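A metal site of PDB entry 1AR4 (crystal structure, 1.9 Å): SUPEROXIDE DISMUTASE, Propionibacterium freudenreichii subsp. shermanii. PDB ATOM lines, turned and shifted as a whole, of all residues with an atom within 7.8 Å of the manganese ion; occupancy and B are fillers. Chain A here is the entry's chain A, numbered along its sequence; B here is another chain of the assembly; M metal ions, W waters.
The manganese ion is bound by OD2 of Asp 161, NE2 of His 27, NE2 of His 75, NE2 of His 165 and water W1.
O of Gly 71 lies within hydrogen-bond range of ND1 of His 75, 2.6 Å away. OH of Tyr 178 lies within hydrogen-bond range of O of Asp 161 (2.9 Å). The indole nitrogen (NE1) of Trp 79 lies close to the backbone carbonyl oxygen (O) of His 75 (3.4 Å). The backbone NH (N) of His 32 is in hydrogen-bond range of the backbone carbonyl oxygen (O) of His 27. OE2 of Glu 164 of chain B is in hydrogen-bond range of ND1 of His 165. The side-chain carboxylate (OD1) of Asp 161 is in hydrogen-bond range of the backbone NH (N) of Trp 163, 3.1 Å away.
Water W1 lies within hydrogen-bond range of the side-chain carboxylate (OD1) of Asp 161 (2.9 Å) and a ring nitrogen (NE2) of His 146 (3.2 Å).
Within 4 Å of the manganese ion: His 27, His 75, Asp 161 and His 165.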
ATOM      1  N   HIS A  27      37.318   3.193   0.057  1.00  0.00           N
ATOM      2  CA  HIS A  27      35.897   2.966   0.209  1.00  0.00           C
ATOM      3  C   HIS A  27      35.445   2.956   1.659  1.00  0.00           C
ATOM      4  O   HIS A  27      34.452   3.576   2.022  1.00  0.00           O
ATOM      5  CB  HIS A  27      35.532   1.637  -0.454  1.00  0.00           C
ATOM      6  CG  HIS A  27      34.108   1.527  -0.881  1.00  0.00           C
ATOM      7  ND1 HIS A  27      33.596   0.392  -1.461  1.00  0.00           N
ATOM      8  CD2 HIS A  27      33.081   2.424  -0.821  1.00  0.00           C
ATOM      9  CE1 HIS A  27      32.311   0.579  -1.745  1.00  0.00           C
ATOM     10  NE2 HIS A  27      31.980   1.809  -1.362  1.00  0.00           N
ATOM     11  N   HIS A  28      36.203   2.268   2.514  1.00  0.00           N
ATOM     12  CA  HIS A  28      35.869   2.171   3.919  1.00  0.00           C
ATOM     13  C   HIS A  28      36.320   3.362   4.763  1.00  0.00           C
ATOM     14  O   HIS A  28      35.504   4.006   5.432  1.00  0.00           O
ATOM     15  CB  HIS A  28      36.454   0.881   4.509  1.00  0.00           C
ATOM     16  CG  HIS A  28      36.205   0.719   5.977  1.00  0.00           C
ATOM     17  ND1 HIS A  28      35.117   0.055   6.476  1.00  0.00           N
ATOM     18  CD2 HIS A  28      36.904   1.175   7.048  1.00  0.00           C
ATOM     19  CE1 HIS A  28      35.144   0.103   7.798  1.00  0.00           C
ATOM     20  NE2 HIS A  28      36.212   0.770   8.166  1.00  0.00           N
ATOM     21  N   HIS A  31      35.064   7.117   2.202  1.00  0.00           N
ATOM     22  CA  HIS A  31      33.653   7.234   1.833  1.00  0.00           C
ATOM     23  C   HIS A  31      32.665   6.861   2.930  1.00  0.00           C
ATOM     24  O   HIS A  31      31.732   7.620   3.200  1.00  0.00           O
ATOM     25  CB  HIS A  31      33.364   6.425   0.563  1.00  0.00           C
ATOM     26  CG  HIS A  31      33.974   7.018  -0.672  1.00  0.00           C
ATOM     27  ND1 HIS A  31      35.142   6.558  -1.222  1.00  0.00           N
ATOM     28  CD2 HIS A  31      33.568   8.047  -1.451  1.00  0.00           C
ATOM     29  CE1 HIS A  31      35.446   7.288  -2.285  1.00  0.00           C
ATOM     30  NE2 HIS A  31      34.503   8.194  -2.444  1.00  0.00           N
ATOM     31  N   HIS A  32      32.863   5.703   3.551  1.00  0.00           N
ATOM     32  CA  HIS A  32      31.956   5.263   4.611  1.00  0.00           C
ATOM     33  C   HIS A  32      32.037   6.192   5.825  1.00  0.00           C
ATOM     34  O   HIS A  32      31.013   6.569   6.389  1.00  0.00           O
ATOM     35  CB  HIS A  32      32.225   3.813   5.015  1.00  0.00           C
ATOM     36  CG  HIS A  32      31.124   3.186   5.822  1.00  0.00           C
ATOM     37  ND1 HIS A  32      31.184   1.886   6.273  1.00  0.00           N
ATOM     38  CD2 HIS A  32      29.940   3.683   6.237  1.00  0.00           C
ATOM     39  CE1 HIS A  32      30.079   1.610   6.944  1.00  0.00           C
ATOM     40  NE2 HIS A  32      29.307   2.688   6.943  1.00  0.00           N
ATOM     41  N   TYR A  35      29.870   9.224   5.463  1.00  0.00           N
ATOM     42  CA  TYR A  35      28.432   9.029   5.677  1.00  0.00           C
ATOM     43  C   TYR A  35      28.114   8.990   7.166  1.00  0.00           C
ATOM     44  O   TYR A  35      27.104   9.531   7.600  1.00  0.00           O
ATOM     45  CB  TYR A  35      27.937   7.760   4.975  1.00  0.00           C
ATOM     46  CG  TYR A  35      28.189   7.780   3.489  1.00  0.00           C
ATOM     47  CD1 TYR A  35      27.824   8.882   2.708  1.00  0.00           C
ATOM     48  CD2 TYR A  35      28.830   6.712   2.863  1.00  0.00           C
ATOM     49  CE1 TYR A  35      28.104   8.927   1.348  1.00  0.00           C
ATOM     50  CE2 TYR A  35      29.113   6.744   1.501  1.00  0.00           C
ATOM     51  CZ  TYR A  35      28.742   7.849   0.749  1.00  0.00           C
ATOM     52  OH  TYR A  35      29.025   7.878  -0.595  1.00  0.00           O
ATOM     53  N   GLY A  71      23.580   5.706   3.355  1.00  0.00           N
ATOM     54  CA  GLY A  71      24.948   5.374   2.951  1.00  0.00           C
ATOM     55  C   GLY A  71      25.646   4.533   4.001  1.00  0.00           C
ATOM     56  O   GLY A  71      26.386   3.614   3.674  1.00  0.00           O
ATOM     57  N   ASN A  74      23.819   0.948   3.986  1.00  0.00           N
ATOM     58  CA  ASN A  74      24.198   0.222   2.784  1.00  0.00           C
ATOM     59  C   ASN A  74      25.635  -0.304   2.821  1.00  0.00           C
ATOM     60  O   ASN A  74      25.891  -1.451   2.472  1.00  0.00           O
ATOM     61  CB  ASN A  74      23.991   1.095   1.538  1.00  0.00           C
ATOM     62  CG  ASN A  74      22.527   1.414   1.265  1.00  0.00           C
ATOM     63  OD1 ASN A  74      21.630   0.858   1.891  1.00  0.00           O
ATOM     64  ND2 ASN A  74      22.288   2.295   0.305  1.00  0.00           N
ATOM     65  N   HIS A  75      26.572   0.540   3.251  1.00  0.00           N
ATOM     66  CA  HIS A  75      27.968   0.131   3.332  1.00  0.00           C
ATOM     67  C   HIS A  75      28.213  -0.858   4.459  1.00  0.00           C
ATOM     68  O   HIS A  75      28.982  -1.799   4.292  1.00  0.00           O
ATOM     69  CB  HIS A  75      28.889   1.349   3.473  1.00  0.00           C
ATOM     70  CG  HIS A  75      29.037   2.127   2.200  1.00  0.00           C
ATOM     71  ND1 HIS A  75      28.153   3.114   1.831  1.00  0.00           N
ATOM     72  CD2 HIS A  75      29.964   2.053   1.214  1.00  0.00           C
ATOM     73  CE1 HIS A  75      28.524   3.616   0.664  1.00  0.00           C
ATOM     74  NE2 HIS A  75      29.607   2.983   0.265  1.00  0.00           N
ATOM     75  N   PHE A  78      27.135  -4.048   3.150  1.00  0.00           N
ATOM     76  CA  PHE A  78      28.062  -4.394   2.071  1.00  0.00           C
ATOM     77  C   PHE A  78      29.334  -5.115   2.536  1.00  0.00           C
ATOM     78  O   PHE A  78      29.740  -6.108   1.940  1.00  0.00           O
ATOM     79  CB  PHE A  78      28.405  -3.125   1.288  1.00  0.00           C
ATOM     80  CG  PHE A  78      29.171  -3.354   0.019  1.00  0.00           C
ATOM     81  CD1 PHE A  78      28.660  -4.181  -0.982  1.00  0.00           C
ATOM     82  CD2 PHE A  78      30.398  -2.750  -0.191  1.00  0.00           C
ATOM     83  CE1 PHE A  78      29.361  -4.389  -2.173  1.00  0.00           C
ATOM     84  CE2 PHE A  78      31.107  -2.935  -1.379  1.00  0.00           C
ATOM     85  CZ  PHE A  78      30.589  -3.765  -2.374  1.00  0.00           C
ATOM     86  N   TRP A  79      29.953  -4.608   3.601  1.00  0.00           N
ATOM     87  CA  TRP A  79      31.190  -5.201   4.141  1.00  0.00           C
ATOM     88  C   TRP A  79      30.971  -6.639   4.618  1.00  0.00           C
ATOM     89  O   TRP A  79      31.770  -7.521   4.319  1.00  0.00           O
ATOM     90  CB  TRP A  79      31.736  -4.373   5.305  1.00  0.00           C
ATOM     91  CG  TRP A  79      31.956  -2.909   5.023  1.00  0.00           C
ATOM     92  CD1 TRP A  79      31.717  -1.873   5.882  1.00  0.00           C
ATOM     93  CD2 TRP A  79      32.466  -2.324   3.822  1.00  0.00           C
ATOM     94  NE1 TRP A  79      32.048  -0.682   5.286  1.00  0.00           N
ATOM     95  CE2 TRP A  79      32.511  -0.919   4.026  1.00  0.00           C
ATOM     96  CE3 TRP A  79      32.902  -2.839   2.589  1.00  0.00           C
ATOM     97  CZ2 TRP A  79      32.962  -0.033   3.043  1.00  0.00           C
ATOM     98  CZ3 TRP A  79      33.356  -1.946   1.613  1.00  0.00           C
ATOM     99  CH2 TRP A  79      33.379  -0.563   1.849  1.00  0.00           C
ATOM    100  N   GLY A 125      24.044   4.071  -7.602  1.00  0.00           N
ATOM    101  CA  GLY A 125      23.025   3.228  -7.020  1.00  0.00           C
ATOM    102  C   GLY A 125      23.488   1.890  -6.467  1.00  0.00           C
ATOM    103  O   GLY A 125      24.678   1.603  -6.401  1.00  0.00           O
ATOM    104  N   TRP A 126      22.507   1.071  -6.073  1.00  0.00           N
ATOM    105  CA  TRP A 126      22.761  -0.243  -5.506  1.00  0.00           C
ATOM    106  C   TRP A 126      21.809  -1.290  -6.079  1.00  0.00           C
ATOM    107  O   TRP A 126      20.698  -0.973  -6.490  1.00  0.00           O
ATOM    108  CB  TRP A 126      22.552  -0.251  -3.990  1.00  0.00           C
ATOM    109  CG  TRP A 126      23.446   0.650  -3.215  1.00  0.00           C
ATOM    110  CD1 TRP A 126      23.412   2.017  -3.179  1.00  0.00           C
ATOM    111  CD2 TRP A 126      24.524   0.255  -2.355  1.00  0.00           C
ATOM    112  NE1 TRP A 126      24.401   2.496  -2.365  1.00  0.00           N
ATOM    113  CE2 TRP A 126      25.100   1.433  -1.844  1.00  0.00           C
ATOM    114  CE3 TRP A 126      25.060  -0.981  -1.979  1.00  0.00           C
ATOM    115  CZ2 TRP A 126      26.192   1.423  -0.969  1.00  0.00           C
ATOM    116  CZ3 TRP A 126      26.141  -1.000  -1.106  1.00  0.00           C
ATOM    117  CH2 TRP A 126      26.699   0.191  -0.617  1.00  0.00           C
ATOM    118  N   HIS A 146      21.662   6.345  -2.539  1.00  0.00           N
ATOM    119  CA  HIS A 146      21.675   5.459  -1.366  1.00  0.00           C
ATOM    120  C   HIS A 146      20.280   5.282  -0.771  1.00  0.00           C
ATOM    121  O   HIS A 146      19.953   4.217  -0.247  1.00  0.00           O
ATOM    122  CB  HIS A 146      22.523   6.059  -0.235  1.00  0.00           C
ATOM    123  CG  HIS A 146      23.990   6.086  -0.510  1.00  0.00           C
ATOM    124  ND1 HIS A 146      24.784   7.178  -0.189  1.00  0.00           N
ATOM    125  CD2 HIS A 146      24.812   5.166  -1.047  1.00  0.00           C
ATOM    126  CE1 HIS A 146      26.029   6.916  -0.527  1.00  0.00           C
ATOM    127  NE2 HIS A 146      26.078   5.708  -1.060  1.00  0.00           N
ATOM    128  N   ASP A 161      27.289  -2.504  -4.218  1.00  0.00           N
ATOM    129  CA  ASP A 161      27.506  -1.076  -4.446  1.00  0.00           C
ATOM    130  C   ASP A 161      27.846  -0.826  -5.907  1.00  0.00           C
ATOM    131  O   ASP A 161      28.859  -1.308  -6.403  1.00  0.00           O
ATOM    132  CB  ASP A 161      28.644  -0.586  -3.553  1.00  0.00           C
ATOM    133  CG  ASP A 161      28.738   0.935  -3.503  1.00  0.00           C
ATOM    134  OD1 ASP A 161      27.984   1.642  -4.216  1.00  0.00           O
ATOM    135  OD2 ASP A 161      29.568   1.430  -2.717  1.00  0.00           O
ATOM    136  N   MET A 162      26.998  -0.067  -6.591  1.00  0.00           N
ATOM    137  CA  MET A 162      27.224   0.255  -7.991  1.00  0.00           C
ATOM    138  C   MET A 162      27.673   1.689  -8.258  1.00  0.00           C
ATOM    139  O   MET A 162      27.624   2.165  -9.396  1.00  0.00           O
ATOM    140  CB  MET A 162      26.018  -0.106  -8.856  1.00  0.00           C
ATOM    141  CG  MET A 162      25.818  -1.616  -9.040  1.00  0.00           C
ATOM    142  SD  MET A 162      27.304  -2.477  -9.616  1.00  0.00           S
ATOM    143  CE  MET A 162      27.502  -1.775 -11.247  1.00  0.00           C
ATOM    144  N   TRP A 163      28.081   2.388  -7.204  1.00  0.00           N
ATOM    145  CA  TRP A 163      28.612   3.742  -7.346  1.00  0.00           C
ATOM    146  C   TRP A 163      29.966   3.551  -8.024  1.00  0.00           C
ATOM    147  O   TRP A 163      30.643   2.560  -7.761  1.00  0.00           O
ATOM    148  CB  TRP A 163      28.822   4.400  -5.980  1.00  0.00           C
ATOM    149  CG  TRP A 163      27.590   4.969  -5.352  1.00  0.00           C
ATOM    150  CD1 TRP A 163      26.407   4.319  -5.113  1.00  0.00           C
ATOM    151  CD2 TRP A 163      27.418   6.304  -4.873  1.00  0.00           C
ATOM    152  NE1 TRP A 163      25.518   5.169  -4.522  1.00  0.00           N
ATOM    153  CE2 TRP A 163      26.100   6.400  -4.365  1.00  0.00           C
ATOM    154  CE3 TRP A 163      28.233   7.443  -4.831  1.00  0.00           C
ATOM    155  CZ2 TRP A 163      25.585   7.581  -3.816  1.00  0.00           C
ATOM    156  CZ3 TRP A 163      27.732   8.619  -4.283  1.00  0.00           C
ATOM    157  CH2 TRP A 163      26.408   8.678  -3.779  1.00  0.00           C
ATOM    158  N   GLU A 164      30.365   4.489  -8.861  1.00  0.00           N
ATOM    159  CA  GLU A 164      31.640   4.374  -9.569  1.00  0.00           C
ATOM    160  C   GLU A 164      32.870   4.242  -8.668  1.00  0.00           C
ATOM    161  O   GLU A 164      33.820   3.564  -9.027  1.00  0.00           O
ATOM    162  CB  GLU A 164      31.793   5.506 -10.599  1.00  0.00           C
ATOM    163  CG  GLU A 164      30.718   5.437 -11.682  1.00  0.00           C
ATOM    164  CD  GLU A 164      30.734   6.581 -12.670  1.00  0.00           C
ATOM    165  OE1 GLU A 164      30.942   7.744 -12.251  1.00  0.00           O
ATOM    166  OE2 GLU A 164      30.521   6.330 -13.874  1.00  0.00           O
ATOM    167  N   HIS A 165      32.839   4.847  -7.479  1.00  0.00           N
ATOM    168  CA  HIS A 165      33.967   4.746  -6.569  1.00  0.00           C
ATOM    169  C   HIS A 165      34.206   3.328  -6.068  1.00  0.00           C
ATOM    170  O   HIS A 165      35.281   3.004  -5.548  1.00  0.00           O
ATOM    171  CB  HIS A 165      33.833   5.723  -5.380  1.00  0.00           C
ATOM    172  CG  HIS A 165      32.710   5.410  -4.439  1.00  0.00           C
ATOM    173  ND1 HIS A 165      31.705   6.306  -4.164  1.00  0.00           N
ATOM    174  CD2 HIS A 165      32.471   4.334  -3.642  1.00  0.00           C
ATOM    175  CE1 HIS A 165      30.892   5.808  -3.244  1.00  0.00           C
ATOM    176  NE2 HIS A 165      31.341   4.604  -2.912  1.00  0.00           N
ATOM    177  N   ALA A 166      33.205   2.467  -6.233  1.00  0.00           N
ATOM    178  CA  ALA A 166      33.311   1.081  -5.788  1.00  0.00           C
ATOM    179  C   ALA A 166      34.096   0.184  -6.735  1.00  0.00           C
ATOM    180  O   ALA A 166      34.619  -0.857  -6.317  1.00  0.00           O
ATOM    181  CB  ALA A 166      31.917   0.494  -5.560  1.00  0.00           C
ATOM    182  N   PHE A 167      34.246   0.597  -7.990  1.00  0.00           N
ATOM    183  CA  PHE A 167      34.940  -0.236  -8.953  1.00  0.00           C
ATOM    184  C   PHE A 167      35.853   0.431  -9.966  1.00  0.00           C
ATOM    185  O   PHE A 167      36.690  -0.224 -10.573  1.00  0.00           O
ATOM    186  CB  PHE A 167      33.918  -1.075  -9.727  1.00  0.00           C
ATOM    187  CG  PHE A 167      32.897  -0.248 -10.473  1.00  0.00           C
ATOM    188  CD1 PHE A 167      33.162   0.241 -11.747  1.00  0.00           C
ATOM    189  CD2 PHE A 167      31.653   0.036  -9.905  1.00  0.00           C
ATOM    190  CE1 PHE A 167      32.231   0.999 -12.443  1.00  0.00           C
ATOM    191  CE2 PHE A 167      30.706   0.790 -10.590  1.00  0.00           C
ATOM    192  CZ  PHE A 167      30.989   1.267 -11.859  1.00  0.00           C
ATOM    193  N   TYR A 178      33.131  -6.155 -13.028  1.00  0.00           N
ATOM    194  CA  TYR A 178      33.096  -5.909 -11.588  1.00  0.00           C
ATOM    195  C   TYR A 178      32.041  -6.800 -10.913  1.00  0.00           C
ATOM    196  O   TYR A 178      32.323  -7.433  -9.898  1.00  0.00           O
ATOM    197  CB  TYR A 178      32.809  -4.432 -11.313  1.00  0.00           C
ATOM    198  CG  TYR A 178      32.359  -4.109  -9.907  1.00  0.00           C
ATOM    199  CD1 TYR A 178      33.140  -4.454  -8.804  1.00  0.00           C
ATOM    200  CD2 TYR A 178      31.161  -3.439  -9.680  1.00  0.00           C
ATOM    201  CE1 TYR A 178      32.744  -4.136  -7.504  1.00  0.00           C
ATOM    202  CE2 TYR A 178      30.751  -3.115  -8.396  1.00  0.00           C
ATOM    203  CZ  TYR A 178      31.547  -3.462  -7.310  1.00  0.00           C
ATOM    204  OH  TYR A 178      31.150  -3.120  -6.035  1.00  0.00           O
ATOM    205  N   GLU B 164      31.799  10.595 -10.493  1.00  0.00           N
ATOM    206  CA  GLU B 164      33.070  10.025 -10.078  1.00  0.00           C
ATOM    207  C   GLU B 164      33.994   9.592 -11.215  1.00  0.00           C
ATOM    208  O   GLU B 164      35.212   9.746 -11.093  1.00  0.00           O
ATOM    209  CB  GLU B 164      32.843   8.895  -9.067  1.00  0.00           C
ATOM    210  CG  GLU B 164      32.262   9.438  -7.762  1.00  0.00           C
ATOM    211  CD  GLU B 164      31.899   8.350  -6.769  1.00  0.00           C
ATOM    212  OE1 GLU B 164      31.421   7.273  -7.185  1.00  0.00           O
ATOM    213  OE2 GLU B 164      32.093   8.590  -5.561  1.00  0.00           O
HETATM  214 MN    MN M   1      30.257   2.982  -1.831  1.00  0.00          MN
HETATM  215  O   HOH W   1      28.322   3.908  -2.513  1.00  0.00           O
